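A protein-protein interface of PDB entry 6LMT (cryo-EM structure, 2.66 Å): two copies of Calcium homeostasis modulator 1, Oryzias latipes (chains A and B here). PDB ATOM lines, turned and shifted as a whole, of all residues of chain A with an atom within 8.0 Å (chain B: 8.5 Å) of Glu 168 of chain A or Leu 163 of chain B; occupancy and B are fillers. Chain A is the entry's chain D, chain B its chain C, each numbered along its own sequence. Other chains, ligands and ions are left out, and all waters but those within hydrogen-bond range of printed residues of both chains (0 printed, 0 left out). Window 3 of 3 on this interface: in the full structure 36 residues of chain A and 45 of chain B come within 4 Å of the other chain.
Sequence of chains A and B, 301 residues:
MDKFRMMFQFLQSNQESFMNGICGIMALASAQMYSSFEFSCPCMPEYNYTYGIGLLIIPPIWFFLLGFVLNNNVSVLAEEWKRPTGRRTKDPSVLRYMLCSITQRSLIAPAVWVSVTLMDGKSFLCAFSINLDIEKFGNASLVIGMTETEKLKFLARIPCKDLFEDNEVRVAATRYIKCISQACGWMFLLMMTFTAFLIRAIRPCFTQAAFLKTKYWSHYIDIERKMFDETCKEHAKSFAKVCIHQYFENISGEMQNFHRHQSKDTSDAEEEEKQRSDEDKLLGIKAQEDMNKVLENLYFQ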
ATOM      1  N   LYS A 136      21.409   7.986   1.424  1.00  0.00           N
ATOM      2  CA  LYS A 136      21.438   8.316   2.839  1.00  0.00           C
ATOM      3  C   LYS A 136      20.156   8.970   3.327  1.00  0.00           C
ATOM      4  O   LYS A 136      20.080   9.330   4.504  1.00  0.00           O
ATOM      5  CB  LYS A 136      22.604   9.257   3.114  1.00  0.00           C
ATOM      6  CG  LYS A 136      23.963   8.642   2.908  1.00  0.00           C
ATOM      7  CD  LYS A 136      25.027   9.720   2.885  1.00  0.00           C
ATOM      8  CE  LYS A 136      25.182  10.385   4.234  1.00  0.00           C
ATOM      9  NZ  LYS A 136      26.294  11.365   4.224  1.00  0.00           N
ATOM     10  N   PHE A 137      19.157   9.139   2.465  1.00  0.00           N
ATOM     11  CA  PHE A 137      18.071  10.075   2.710  1.00  0.00           C
ATOM     12  C   PHE A 137      16.682   9.485   2.542  1.00  0.00           C
ATOM     13  O   PHE A 137      15.727  10.061   3.069  1.00  0.00           O
ATOM     14  CB  PHE A 137      18.226  11.284   1.774  1.00  0.00           C
ATOM     15  CG  PHE A 137      19.442  12.093   2.062  1.00  0.00           C
ATOM     16  CD1 PHE A 137      19.786  12.395   3.362  1.00  0.00           C
ATOM     17  CD2 PHE A 137      20.338  12.380   1.060  1.00  0.00           C
ATOM     18  CE1 PHE A 137      20.929  13.083   3.639  1.00  0.00           C
ATOM     19  CE2 PHE A 137      21.491  13.050   1.339  1.00  0.00           C
ATOM     20  CZ  PHE A 137      21.783  13.403   2.631  1.00  0.00           C
ATOM     21  N   GLY A 138      16.535   8.369   1.834  1.00  0.00           N
ATOM     22  CA  GLY A 138      15.218   7.805   1.610  1.00  0.00           C
ATOM     23  C   GLY A 138      15.220   6.445   0.952  1.00  0.00           C
ATOM     24  O   GLY A 138      15.988   5.564   1.353  1.00  0.00           O
ATOM     25  N   ASN A 139      14.339   6.255  -0.033  1.00  0.00           N
ATOM     26  CA  ASN A 139      14.356   5.043  -0.842  1.00  0.00           C
ATOM     27  C   ASN A 139      15.665   4.933  -1.610  1.00  0.00           C
ATOM     28  O   ASN A 139      16.263   5.933  -2.017  1.00  0.00           O
ATOM     29  CB  ASN A 139      13.185   5.024  -1.832  1.00  0.00           C
ATOM     30  CG  ASN A 139      11.858   4.656  -1.182  1.00  0.00           C
ATOM     31  OD1 ASN A 139      11.786   3.750  -0.354  1.00  0.00           O
ATOM     32  ND2 ASN A 139      10.795   5.346  -1.578  1.00  0.00           N
ATOM     33  N   LEU A 142      15.041   5.227  -5.886  1.00  0.00           N
ATOM     34  CA  LEU A 142      14.829   6.468  -6.617  1.00  0.00           C
ATOM     35  C   LEU A 142      15.735   6.554  -7.834  1.00  0.00           C
ATOM     36  O   LEU A 142      15.248   6.631  -8.965  1.00  0.00           O
ATOM     37  CB  LEU A 142      15.068   7.669  -5.703  1.00  0.00           C
ATOM     38  CG  LEU A 142      14.085   7.905  -4.563  1.00  0.00           C
ATOM     39  CD1 LEU A 142      14.561   9.059  -3.727  1.00  0.00           C
ATOM     40  CD2 LEU A 142      12.697   8.179  -5.109  1.00  0.00           C
ATOM     41  N   PHE A 164      10.214  18.986  -6.840  1.00  0.00           N
ATOM     42  CA  PHE A 164      10.711  17.737  -6.290  1.00  0.00           C
ATOM     43  C   PHE A 164       9.548  17.115  -5.544  1.00  0.00           C
ATOM     44  O   PHE A 164       8.928  17.775  -4.706  1.00  0.00           O
ATOM     45  CB  PHE A 164      11.901  17.973  -5.360  1.00  0.00           C
ATOM     46  CG  PHE A 164      12.683  16.741  -5.064  1.00  0.00           C
ATOM     47  CD1 PHE A 164      13.638  16.299  -5.947  1.00  0.00           C
ATOM     48  CD2 PHE A 164      12.442  16.005  -3.931  1.00  0.00           C
ATOM     49  CE1 PHE A 164      14.350  15.169  -5.691  1.00  0.00           C
ATOM     50  CE2 PHE A 164      13.152  14.875  -3.677  1.00  0.00           C
ATOM     51  CZ  PHE A 164      14.105  14.460  -4.557  1.00  0.00           C
ATOM     52  N   GLU A 165       9.242  15.858  -5.847  1.00  0.00           N
ATOM     53  CA  GLU A 165       7.976  15.297  -5.401  1.00  0.00           C
ATOM     54  C   GLU A 165       8.089  14.515  -4.098  1.00  0.00           C
ATOM     55  O   GLU A 165       7.139  14.500  -3.310  1.00  0.00           O
ATOM     56  CB  GLU A 165       7.382  14.423  -6.513  1.00  0.00           C
ATOM     57  CG  GLU A 165       8.135  13.132  -6.830  1.00  0.00           C
ATOM     58  CD  GLU A 165       9.279  13.314  -7.821  1.00  0.00           C
ATOM     59  OE1 GLU A 165       9.698  14.466  -8.077  1.00  0.00           O
ATOM     60  OE2 GLU A 165       9.771  12.287  -8.339  1.00  0.00           O
ATOM     61  N   ASP A 166       9.228  13.885  -3.833  1.00  0.00           N
ATOM     62  CA  ASP A 166       9.400  13.066  -2.638  1.00  0.00           C
ATOM     63  C   ASP A 166       9.779  13.993  -1.499  1.00  0.00           C
ATOM     64  O   ASP A 166      10.916  14.431  -1.398  1.00  0.00           O
ATOM     65  CB  ASP A 166      10.458  12.000  -2.884  1.00  0.00           C
ATOM     66  CG  ASP A 166      10.448  10.911  -1.844  1.00  0.00           C
ATOM     67  OD1 ASP A 166       9.713  11.010  -0.844  1.00  0.00           O
ATOM     68  OD2 ASP A 166      11.156   9.910  -2.055  1.00  0.00           O
ATOM     69  N   ASN A 167       8.817  14.295  -0.636  1.00  0.00           N
ATOM     70  CA  ASN A 167       9.032  15.317   0.376  1.00  0.00           C
ATOM     71  C   ASN A 167       9.935  14.813   1.485  1.00  0.00           C
ATOM     72  O   ASN A 167      10.653  15.602   2.093  1.00  0.00           O
ATOM     73  CB  ASN A 167       7.699  15.775   0.958  1.00  0.00           C
ATOM     74  CG  ASN A 167       7.789  17.120   1.635  1.00  0.00           C
ATOM     75  OD1 ASN A 167       8.828  17.769   1.625  1.00  0.00           O
ATOM     76  ND2 ASN A 167       6.691  17.553   2.224  1.00  0.00           N
ATOM     77  N   GLU A 168       9.936  13.510   1.736  1.00  0.00           N
ATOM     78  CA  GLU A 168      10.764  12.957   2.798  1.00  0.00           C
ATOM     79  C   GLU A 168      12.240  13.012   2.436  1.00  0.00           C
ATOM     80  O   GLU A 168      13.074  13.343   3.282  1.00  0.00           O
ATOM     81  CB  GLU A 168      10.314  11.527   3.098  1.00  0.00           C
ATOM     82  CG  GLU A 168      10.980  10.875   4.290  1.00  0.00           C
ATOM     83  CD  GLU A 168      12.204  10.055   3.923  1.00  0.00           C
ATOM     84  OE1 GLU A 168      12.185   9.373   2.880  1.00  0.00           O
ATOM     85  OE2 GLU A 168      13.209  10.127   4.660  1.00  0.00           O
ATOM     86  N   VAL A 169      12.578  12.702   1.190  1.00  0.00           N
ATOM     87  CA  VAL A 169      13.963  12.780   0.747  1.00  0.00           C
ATOM     88  C   VAL A 169      14.408  14.229   0.642  1.00  0.00           C
ATOM     89  O   VAL A 169      15.553  14.565   0.946  1.00  0.00           O
ATOM     90  CB  VAL A 169      14.114  12.021  -0.584  1.00  0.00           C
ATOM     91  CG1 VAL A 169      15.482  12.177  -1.179  1.00  0.00           C
ATOM     92  CG2 VAL A 169      13.856  10.585  -0.351  1.00  0.00           C
ATOM     93  N   ARG A 170      13.497  15.117   0.261  1.00  0.00           N
ATOM     94  CA  ARG A 170      13.837  16.524   0.155  1.00  0.00           C
ATOM     95  C   ARG A 170      14.076  17.140   1.522  1.00  0.00           C
ATOM     96  O   ARG A 170      15.015  17.911   1.690  1.00  0.00           O
ATOM     97  CB  ARG A 170      12.733  17.273  -0.568  1.00  0.00           C
ATOM     98  CG  ARG A 170      13.081  18.682  -0.846  1.00  0.00           C
ATOM     99  CD  ARG A 170      11.912  19.454  -1.346  1.00  0.00           C
ATOM    100  NE  ARG A 170      10.841  19.469  -0.368  1.00  0.00           N
ATOM    101  CZ  ARG A 170      10.783  20.281   0.678  1.00  0.00           C
ATOM    102  NH1 ARG A 170      11.739  21.161   0.901  1.00  0.00           N
ATOM    103  NH2 ARG A 170       9.762  20.209   1.508  1.00  0.00           N
ATOM    104  N   VAL A 171      13.245  16.809   2.507  1.00  0.00           N
ATOM    105  CA  VAL A 171      13.397  17.357   3.851  1.00  0.00           C
ATOM    106  C   VAL A 171      14.668  16.836   4.513  1.00  0.00           C
ATOM    107  O   VAL A 171      15.380  17.584   5.187  1.00  0.00           O
ATOM    108  CB  VAL A 171      12.128  17.058   4.673  1.00  0.00           C
ATOM    109  CG1 VAL A 171      12.340  17.268   6.137  1.00  0.00           C
ATOM    110  CG2 VAL A 171      11.026  17.971   4.236  1.00  0.00           C
ATOM    111  N   ALA A 172      15.007  15.571   4.279  1.00  0.00           N
ATOM    112  CA  ALA A 172      16.214  15.011   4.869  1.00  0.00           C
ATOM    113  C   ALA A 172      17.473  15.585   4.236  1.00  0.00           C
ATOM    114  O   ALA A 172      18.452  15.859   4.935  1.00  0.00           O
ATOM    115  CB  ALA A 172      16.197  13.497   4.744  1.00  0.00           C
ATOM    116  N   ALA A 173      17.469  15.784   2.922  1.00  0.00           N
ATOM    117  CA  ALA A 173      18.631  16.353   2.251  1.00  0.00           C
ATOM    118  C   ALA A 173      18.783  17.837   2.531  1.00  0.00           C
ATOM    119  O   ALA A 173      19.904  18.338   2.588  1.00  0.00           O
ATOM    120  CB  ALA A 173      18.529  16.108   0.751  1.00  0.00           C
ATOM    121  N   THR A 174      17.676  18.549   2.709  1.00  0.00           N
ATOM    122  CA  THR A 174      17.739  19.959   3.053  1.00  0.00           C
ATOM    123  C   THR A 174      18.276  20.164   4.460  1.00  0.00           C
ATOM    124  O   THR A 174      19.060  21.083   4.692  1.00  0.00           O
ATOM    125  CB  THR A 174      16.358  20.580   2.902  1.00  0.00           C
ATOM    126  OG1 THR A 174      15.912  20.375   1.565  1.00  0.00           O
ATOM    127  CG2 THR A 174      16.369  22.056   3.184  1.00  0.00           C
ATOM    128  N   ARG A 175      17.884  19.311   5.406  1.00  0.00           N
ATOM    129  CA  ARG A 175      18.379  19.433   6.771  1.00  0.00           C
ATOM    130  C   ARG A 175      19.848  19.095   6.888  1.00  0.00           C
ATOM    131  O   ARG A 175      20.553  19.700   7.696  1.00  0.00           O
ATOM    132  CB  ARG A 175      17.584  18.540   7.701  1.00  0.00           C
ATOM    133  CG  ARG A 175      16.291  19.116   8.084  1.00  0.00           C
ATOM    134  CD  ARG A 175      15.602  18.183   8.967  1.00  0.00           C
ATOM    135  NE  ARG A 175      14.382  18.748   9.507  1.00  0.00           N
ATOM    136  CZ  ARG A 175      14.323  19.444  10.634  1.00  0.00           C
ATOM    137  NH1 ARG A 175      15.411  19.650  11.341  1.00  0.00           N
ATOM    138  NH2 ARG A 175      13.170  19.911  11.063  1.00  0.00           N
ATOM    139  N   TYR A 176      20.314  18.134   6.102  1.00  0.00           N
ATOM    140  CA  TYR A 176      21.721  17.775   6.103  1.00  0.00           C
ATOM    141  C   TYR A 176      22.593  18.894   5.559  1.00  0.00           C
ATOM    142  O   TYR A 176      23.637  19.204   6.133  1.00  0.00           O
ATOM    143  CB  TYR A 176      21.896  16.491   5.308  1.00  0.00           C
ATOM    144  CG  TYR A 176      23.308  16.092   5.033  1.00  0.00           C
ATOM    145  CD1 TYR A 176      24.150  15.706   6.052  1.00  0.00           C
ATOM    146  CD2 TYR A 176      23.784  16.054   3.745  1.00  0.00           C
ATOM    147  CE1 TYR A 176      25.428  15.326   5.801  1.00  0.00           C
ATOM    148  CE2 TYR A 176      25.061  15.671   3.483  1.00  0.00           C
ATOM    149  CZ  TYR A 176      25.878  15.304   4.517  1.00  0.00           C
ATOM    150  OH  TYR A 176      27.164  14.921   4.263  1.00  0.00           O
ATOM    151  N   CYS B  41      18.264  20.487  12.901  1.00  0.00           N
ATOM    152  CA  CYS B  41      18.894  19.244  13.306  1.00  0.00           C
ATOM    153  C   CYS B  41      19.077  18.348  12.086  1.00  0.00           C
ATOM    154  O   CYS B  41      18.178  18.279  11.246  1.00  0.00           O
ATOM    155  CB  CYS B  41      18.022  18.563  14.362  1.00  0.00           C
ATOM    156  SG  CYS B  41      18.654  17.084  15.161  1.00  0.00           S
ATOM    157  N   PRO B  42      20.234  17.703  11.925  1.00  0.00           N
ATOM    158  CA  PRO B  42      20.462  16.873  10.739  1.00  0.00           C
ATOM    159  C   PRO B  42      19.543  15.682  10.656  1.00  0.00           C
ATOM    160  O   PRO B  42      19.229  15.249   9.544  1.00  0.00           O
ATOM    161  CB  PRO B  42      21.906  16.405  10.920  1.00  0.00           C
ATOM    162  CG  PRO B  42      22.461  17.260  11.908  1.00  0.00           C
ATOM    163  CD  PRO B  42      21.409  17.711  12.797  1.00  0.00           C
ATOM    164  N   CYS B  43      19.105  15.168  11.809  1.00  0.00           N
ATOM    165  CA  CYS B  43      18.318  13.947  11.959  1.00  0.00           C
ATOM    166  C   CYS B  43      19.011  12.745  11.336  1.00  0.00           C
ATOM    167  O   CYS B  43      18.395  11.920  10.669  1.00  0.00           O
ATOM    168  CB  CYS B  43      16.884  14.123  11.457  1.00  0.00           C
ATOM    169  SG  CYS B  43      15.835  14.875  12.717  1.00  0.00           S
ATOM    170  N   MET B  44      20.303  12.638  11.600  1.00  0.00           N
ATOM    171  CA  MET B  44      21.186  11.553  11.240  1.00  0.00           C
ATOM    172  C   MET B  44      21.991  11.181  12.473  1.00  0.00           C
ATOM    173  O   MET B  44      22.454  12.068  13.185  1.00  0.00           O
ATOM    174  CB  MET B  44      22.128  11.973  10.120  1.00  0.00           C
ATOM    175  CG  MET B  44      21.431  12.283   8.837  1.00  0.00           C
ATOM    176  SD  MET B  44      22.488  13.100   7.659  1.00  0.00           S
ATOM    177  CE  MET B  44      23.605  11.787   7.255  1.00  0.00           C
ATOM    178  N   LYS B 153      19.011   5.067  13.233  1.00  0.00           N
ATOM    179  CA  LYS B 153      18.451   5.986  12.252  1.00  0.00           C
ATOM    180  C   LYS B 153      17.016   6.346  12.582  1.00  0.00           C
ATOM    181  O   LYS B 153      16.564   7.444  12.252  1.00  0.00           O
ATOM    182  CB  LYS B 153      18.509   5.386  10.855  1.00  0.00           C
ATOM    183  CG  LYS B 153      19.893   5.220  10.305  1.00  0.00           C
ATOM    184  CD  LYS B 153      19.836   4.647   8.914  1.00  0.00           C
ATOM    185  CE  LYS B 153      21.219   4.382   8.387  1.00  0.00           C
ATOM    186  NZ  LYS B 153      21.167   3.767   7.038  1.00  0.00           N
ATOM    187  N   PHE B 154      16.290   5.429  13.216  1.00  0.00           N
ATOM    188  CA  PHE B 154      14.905   5.678  13.593  1.00  0.00           C
ATOM    189  C   PHE B 154      14.816   6.695  14.725  1.00  0.00           C
ATOM    190  O   PHE B 154      13.997   7.615  14.679  1.00  0.00           O
ATOM    191  CB  PHE B 154      14.257   4.351  13.985  1.00  0.00           C
ATOM    192  CG  PHE B 154      12.829   4.466  14.394  1.00  0.00           C
ATOM    193  CD1 PHE B 154      11.842   4.623  13.451  1.00  0.00           C
ATOM    194  CD2 PHE B 154      12.476   4.407  15.724  1.00  0.00           C
ATOM    195  CE1 PHE B 154      10.536   4.733  13.825  1.00  0.00           C
ATOM    196  CE2 PHE B 154      11.177   4.521  16.100  1.00  0.00           C
ATOM    197  CZ  PHE B 154      10.203   4.680  15.146  1.00  0.00           C
ATOM    198  N   ALA B 156      17.098   8.870  15.531  1.00  0.00           N
ATOM    199  CA  ALA B 156      17.696  10.136  15.156  1.00  0.00           C
ATOM    200  C   ALA B 156      16.710  11.075  14.494  1.00  0.00           C
ATOM    201  O   ALA B 156      16.972  12.271  14.437  1.00  0.00           O
ATOM    202  CB  ALA B 156      18.873   9.900  14.232  1.00  0.00           C
ATOM    203  N   ARG B 157      15.582  10.575  14.010  1.00  0.00           N
ATOM    204  CA  ARG B 157      14.616  11.400  13.311  1.00  0.00           C
ATOM    205  C   ARG B 157      13.535  11.954  14.225  1.00  0.00           C
ATOM    206  O   ARG B 157      12.668  12.682  13.747  1.00  0.00           O
ATOM    207  CB  ARG B 157      13.996  10.604  12.172  1.00  0.00           C
ATOM    208  CG  ARG B 157      15.001  10.220  11.108  1.00  0.00           C
ATOM    209  CD  ARG B 157      14.345   9.680   9.860  1.00  0.00           C
ATOM    210  NE  ARG B 157      13.661   8.408  10.078  1.00  0.00           N
ATOM    211  CZ  ARG B 157      14.202   7.211   9.862  1.00  0.00           C
ATOM    212  NH1 ARG B 157      15.440   7.106   9.399  1.00  0.00           N
ATOM    213  NH2 ARG B 157      13.498   6.113  10.088  1.00  0.00           N
ATOM    214  N   ILE B 158      13.594  11.612  15.520  1.00  0.00           N
ATOM    215  CA  ILE B 158      12.673  12.203  16.508  1.00  0.00           C
ATOM    216  C   ILE B 158      12.665  13.727  16.562  1.00  0.00           C
ATOM    217  O   ILE B 158      11.569  14.300  16.656  1.00  0.00           O
ATOM    218  CB  ILE B 158      12.901  11.551  17.881  1.00  0.00           C
ATOM    219  CG1 ILE B 158      12.398  10.116  17.866  1.00  0.00           C
ATOM    220  CG2 ILE B 158      12.256  12.307  19.025  1.00  0.00           C
ATOM    221  CD1 ILE B 158      12.749   9.324  19.068  1.00  0.00           C
ATOM    222  N   PRO B 159      13.790  14.462  16.458  1.00  0.00           N
ATOM    223  CA  PRO B 159      13.677  15.929  16.441  1.00  0.00           C
ATOM    224  C   PRO B 159      12.994  16.522  15.218  1.00  0.00           C
ATOM    225  O   PRO B 159      12.755  17.730  15.203  1.00  0.00           O
ATOM    226  CB  PRO B 159      15.128  16.387  16.506  1.00  0.00           C
ATOM    227  CG  PRO B 159      15.820  15.333  17.062  1.00  0.00           C
ATOM    228  CD  PRO B 159      15.215  14.108  16.603  1.00  0.00           C
ATOM    229  N   CYS B 160      12.675  15.733  14.209  1.00  0.00           N
ATOM    230  CA  CYS B 160      12.124  16.202  12.947  1.00  0.00           C
ATOM    231  C   CYS B 160      10.686  15.713  12.845  1.00  0.00           C
ATOM    232  O   CYS B 160      10.445  14.507  12.804  1.00  0.00           O
ATOM    233  CB  CYS B 160      12.979  15.678  11.799  1.00  0.00           C
ATOM    234  SG  CYS B 160      14.702  16.270  11.817  1.00  0.00           S
ATOM    235  N   LYS B 161       9.731  16.647  12.824  1.00  0.00           N
ATOM    236  CA  LYS B 161       8.318  16.276  12.764  1.00  0.00           C
ATOM    237  C   LYS B 161       7.965  15.633  11.436  1.00  0.00           C
ATOM    238  O   LYS B 161       7.200  14.666  11.389  1.00  0.00           O
ATOM    239  CB  LYS B 161       7.426  17.493  12.962  1.00  0.00           C
ATOM    240  CG  LYS B 161       7.522  18.151  14.298  1.00  0.00           C
ATOM    241  CD  LYS B 161       6.544  19.299  14.380  1.00  0.00           C
ATOM    242  CE  LYS B 161       6.614  19.984  15.728  1.00  0.00           C
ATOM    243  NZ  LYS B 161       7.904  20.699  15.913  1.00  0.00           N
ATOM    244  N   ASP B 162       8.497  16.168  10.351  1.00  0.00           N
ATOM    245  CA  ASP B 162       8.204  15.716   9.006  1.00  0.00           C
ATOM    246  C   ASP B 162       9.107  14.587   8.540  1.00  0.00           C
ATOM    247  O   ASP B 162       9.101  14.259   7.354  1.00  0.00           O
ATOM    248  CB  ASP B 162       8.268  16.910   8.057  1.00  0.00           C
ATOM    249  CG  ASP B 162       9.502  17.768   8.273  1.00  0.00           C
ATOM    250  OD1 ASP B 162      10.361  17.423   9.113  1.00  0.00           O
ATOM    251  OD2 ASP B 162       9.592  18.836   7.631  1.00  0.00           O
ATOM    252  N   LEU B 163       9.863  13.973   9.440  1.00  0.00           N
ATOM    253  CA  LEU B 163      10.618  12.775   9.130  1.00  0.00           C
ATOM    254  C   LEU B 163      10.311  11.642  10.088  1.00  0.00           C
ATOM    255  O   LEU B 163      10.837  10.543   9.909  1.00  0.00           O
ATOM    256  CB  LEU B 163      12.127  13.049   9.161  1.00  0.00           C
ATOM    257  CG  LEU B 163      12.724  14.015   8.149  1.00  0.00           C
ATOM    258  CD1 LEU B 163      14.184  14.191   8.413  1.00  0.00           C
ATOM    259  CD2 LEU B 163      12.495  13.518   6.754  1.00  0.00           C
ATOM    260  N   PHE B 164       9.502  11.883  11.110  1.00  0.00           N
ATOM    261  CA  PHE B 164       9.141  10.877  12.092  1.00  0.00           C
ATOM    262  C   PHE B 164       7.630  10.760  12.039  1.00  0.00           C
ATOM    263  O   PHE B 164       6.930  11.770  12.133  1.00  0.00           O
ATOM    264  CB  PHE B 164       9.615  11.271  13.491  1.00  0.00           C
ATOM    265  CG  PHE B 164       9.616  10.142  14.462  1.00  0.00           C
ATOM    266  CD1 PHE B 164      10.672   9.265  14.501  1.00  0.00           C
ATOM    267  CD2 PHE B 164       8.553   9.932  15.304  1.00  0.00           C
ATOM    268  CE1 PHE B 164      10.679   8.225  15.378  1.00  0.00           C
ATOM    269  CE2 PHE B 164       8.559   8.891  16.178  1.00  0.00           C
ATOM    270  CZ  PHE B 164       9.622   8.041  16.214  1.00  0.00           C
ATOM    271  N   GLU B 165       7.128   9.540  11.878  1.00  0.00           N
ATOM    272  CA  GLU B 165       5.725   9.380  11.522  1.00  0.00           C
ATOM    273  C   GLU B 165       4.822   9.143  12.727  1.00  0.00           C
ATOM    274  O   GLU B 165       3.662   9.564  12.714  1.00  0.00           O
ATOM    275  CB  GLU B 165       5.582   8.248  10.497  1.00  0.00           C
ATOM    276  CG  GLU B 165       5.879   6.837  11.007  1.00  0.00           C
ATOM    277  CD  GLU B 165       7.355   6.463  10.957  1.00  0.00           C
ATOM    278  OE1 GLU B 165       8.215   7.359  10.795  1.00  0.00           O
ATOM    279  OE2 GLU B 165       7.656   5.257  11.096  1.00  0.00           O
ATOM    280  N   ASP B 166       5.322   8.500  13.776  1.00  0.00           N
ATOM    281  CA  ASP B 166       4.510   8.177  14.945  1.00  0.00           C
ATOM    282  C   ASP B 166       4.494   9.400  15.841  1.00  0.00           C
ATOM    283  O   ASP B 166       5.454   9.673  16.549  1.00  0.00           O
ATOM    284  CB  ASP B 166       5.076   6.957  15.654  1.00  0.00           C
ATOM    285  CG  ASP B 166       4.117   6.355  16.647  1.00  0.00           C
ATOM    286  OD1 ASP B 166       3.044   6.930  16.904  1.00  0.00           O
ATOM    287  OD2 ASP B 166       4.422   5.256  17.146  1.00  0.00           O
ATOM    288  N   ARG B 170       6.739  10.550  19.280  1.00  0.00           N
ATOM    289  CA  ARG B 170       7.545  11.747  19.126  1.00  0.00           C
ATOM    290  C   ARG B 170       7.189  12.793  20.168  1.00  0.00           C
ATOM    291  O   ARG B 170       8.078  13.424  20.729  1.00  0.00           O
ATOM    292  CB  ARG B 170       7.366  12.320  17.732  1.00  0.00           C
ATOM    293  CG  ARG B 170       8.274  13.453  17.456  1.00  0.00           C
ATOM    294  CD  ARG B 170       7.931  14.139  16.181  1.00  0.00           C
ATOM    295  NE  ARG B 170       6.585  14.680  16.226  1.00  0.00           N
ATOM    296  CZ  ARG B 170       6.250  15.826  16.801  1.00  0.00           C
ATOM    297  NH1 ARG B 170       7.159  16.575  17.392  1.00  0.00           N
ATOM    298  NH2 ARG B 170       4.993  16.223  16.786  1.00  0.00           N
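CE of Lys 136 of chain A touches CE of Met 44 of chain B (3.7 Å). Glu 168 of chain A touches Leu 163 of chain B (O to CD2, 3.5 Å). Val 171 of chain A touches Asp 162 of chain B. Val 171 of chain A touches Leu 163 of chain B (CG1 to CD2, 3.8 Å). Tyr 176 of chain A touches Met 44 of chain B (CD1 to SD, 3.5 Å).
NH1 of Arg 175 of chain A is in hydrogen-bond range of O of Cys 41 of chain B (3.1 Å). The side-chain sulfur (SG) of Cys 160 of chain B sits at hydrogen-bond distance from the guanidinium group (NE) of Arg 175 of chain A, 3.4 Å away.
Positions printed for both chains: 164, 165, 166 and 170. Of the 7 pairs that touch across the chains among the printed residues, none has its exchanged pair printed and touching as well.
SG of Cys 43 of chain B is disulfide-bonded to SG of Cys 160 of chain B, at 2.0 Å.
Glu 168 of chain A touches one residue of chain B. Printed residues of chain B within 4 Å of Arg 175 of chain A: Cys 41 and Cys 160. Of the printed residues of chain A, Cys 41 of chain B touches Arg 175 (3.1 Å). Of the printed residues of chain A, Met 44 of chain B touches Lys 136 (3.7 Å) and Tyr 176 (3.5 Å). Of the printed residues of chain A, Asp 162 of chain B touches Val 171. Of chain A, only Glu 168 and Val 171 come within 4 Å of Leu 163 of chain B. The nearest residue of chain B that does not touch Glu 168 of chain A is Asp 162 of chain B (4.9 Å).
Of the 18 printed residues of chain A, 5 touch a printed residue of chain B. Printed residues of chain A that touch a printed residue of chain B: Lys 136, Glu 168, Val 171, Arg 175 and Tyr 176. Among the printed residues, no Asp or Glu carboxylate lies within 4 Å of a Lys or Arg side-chain nitrogen of the other chain.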
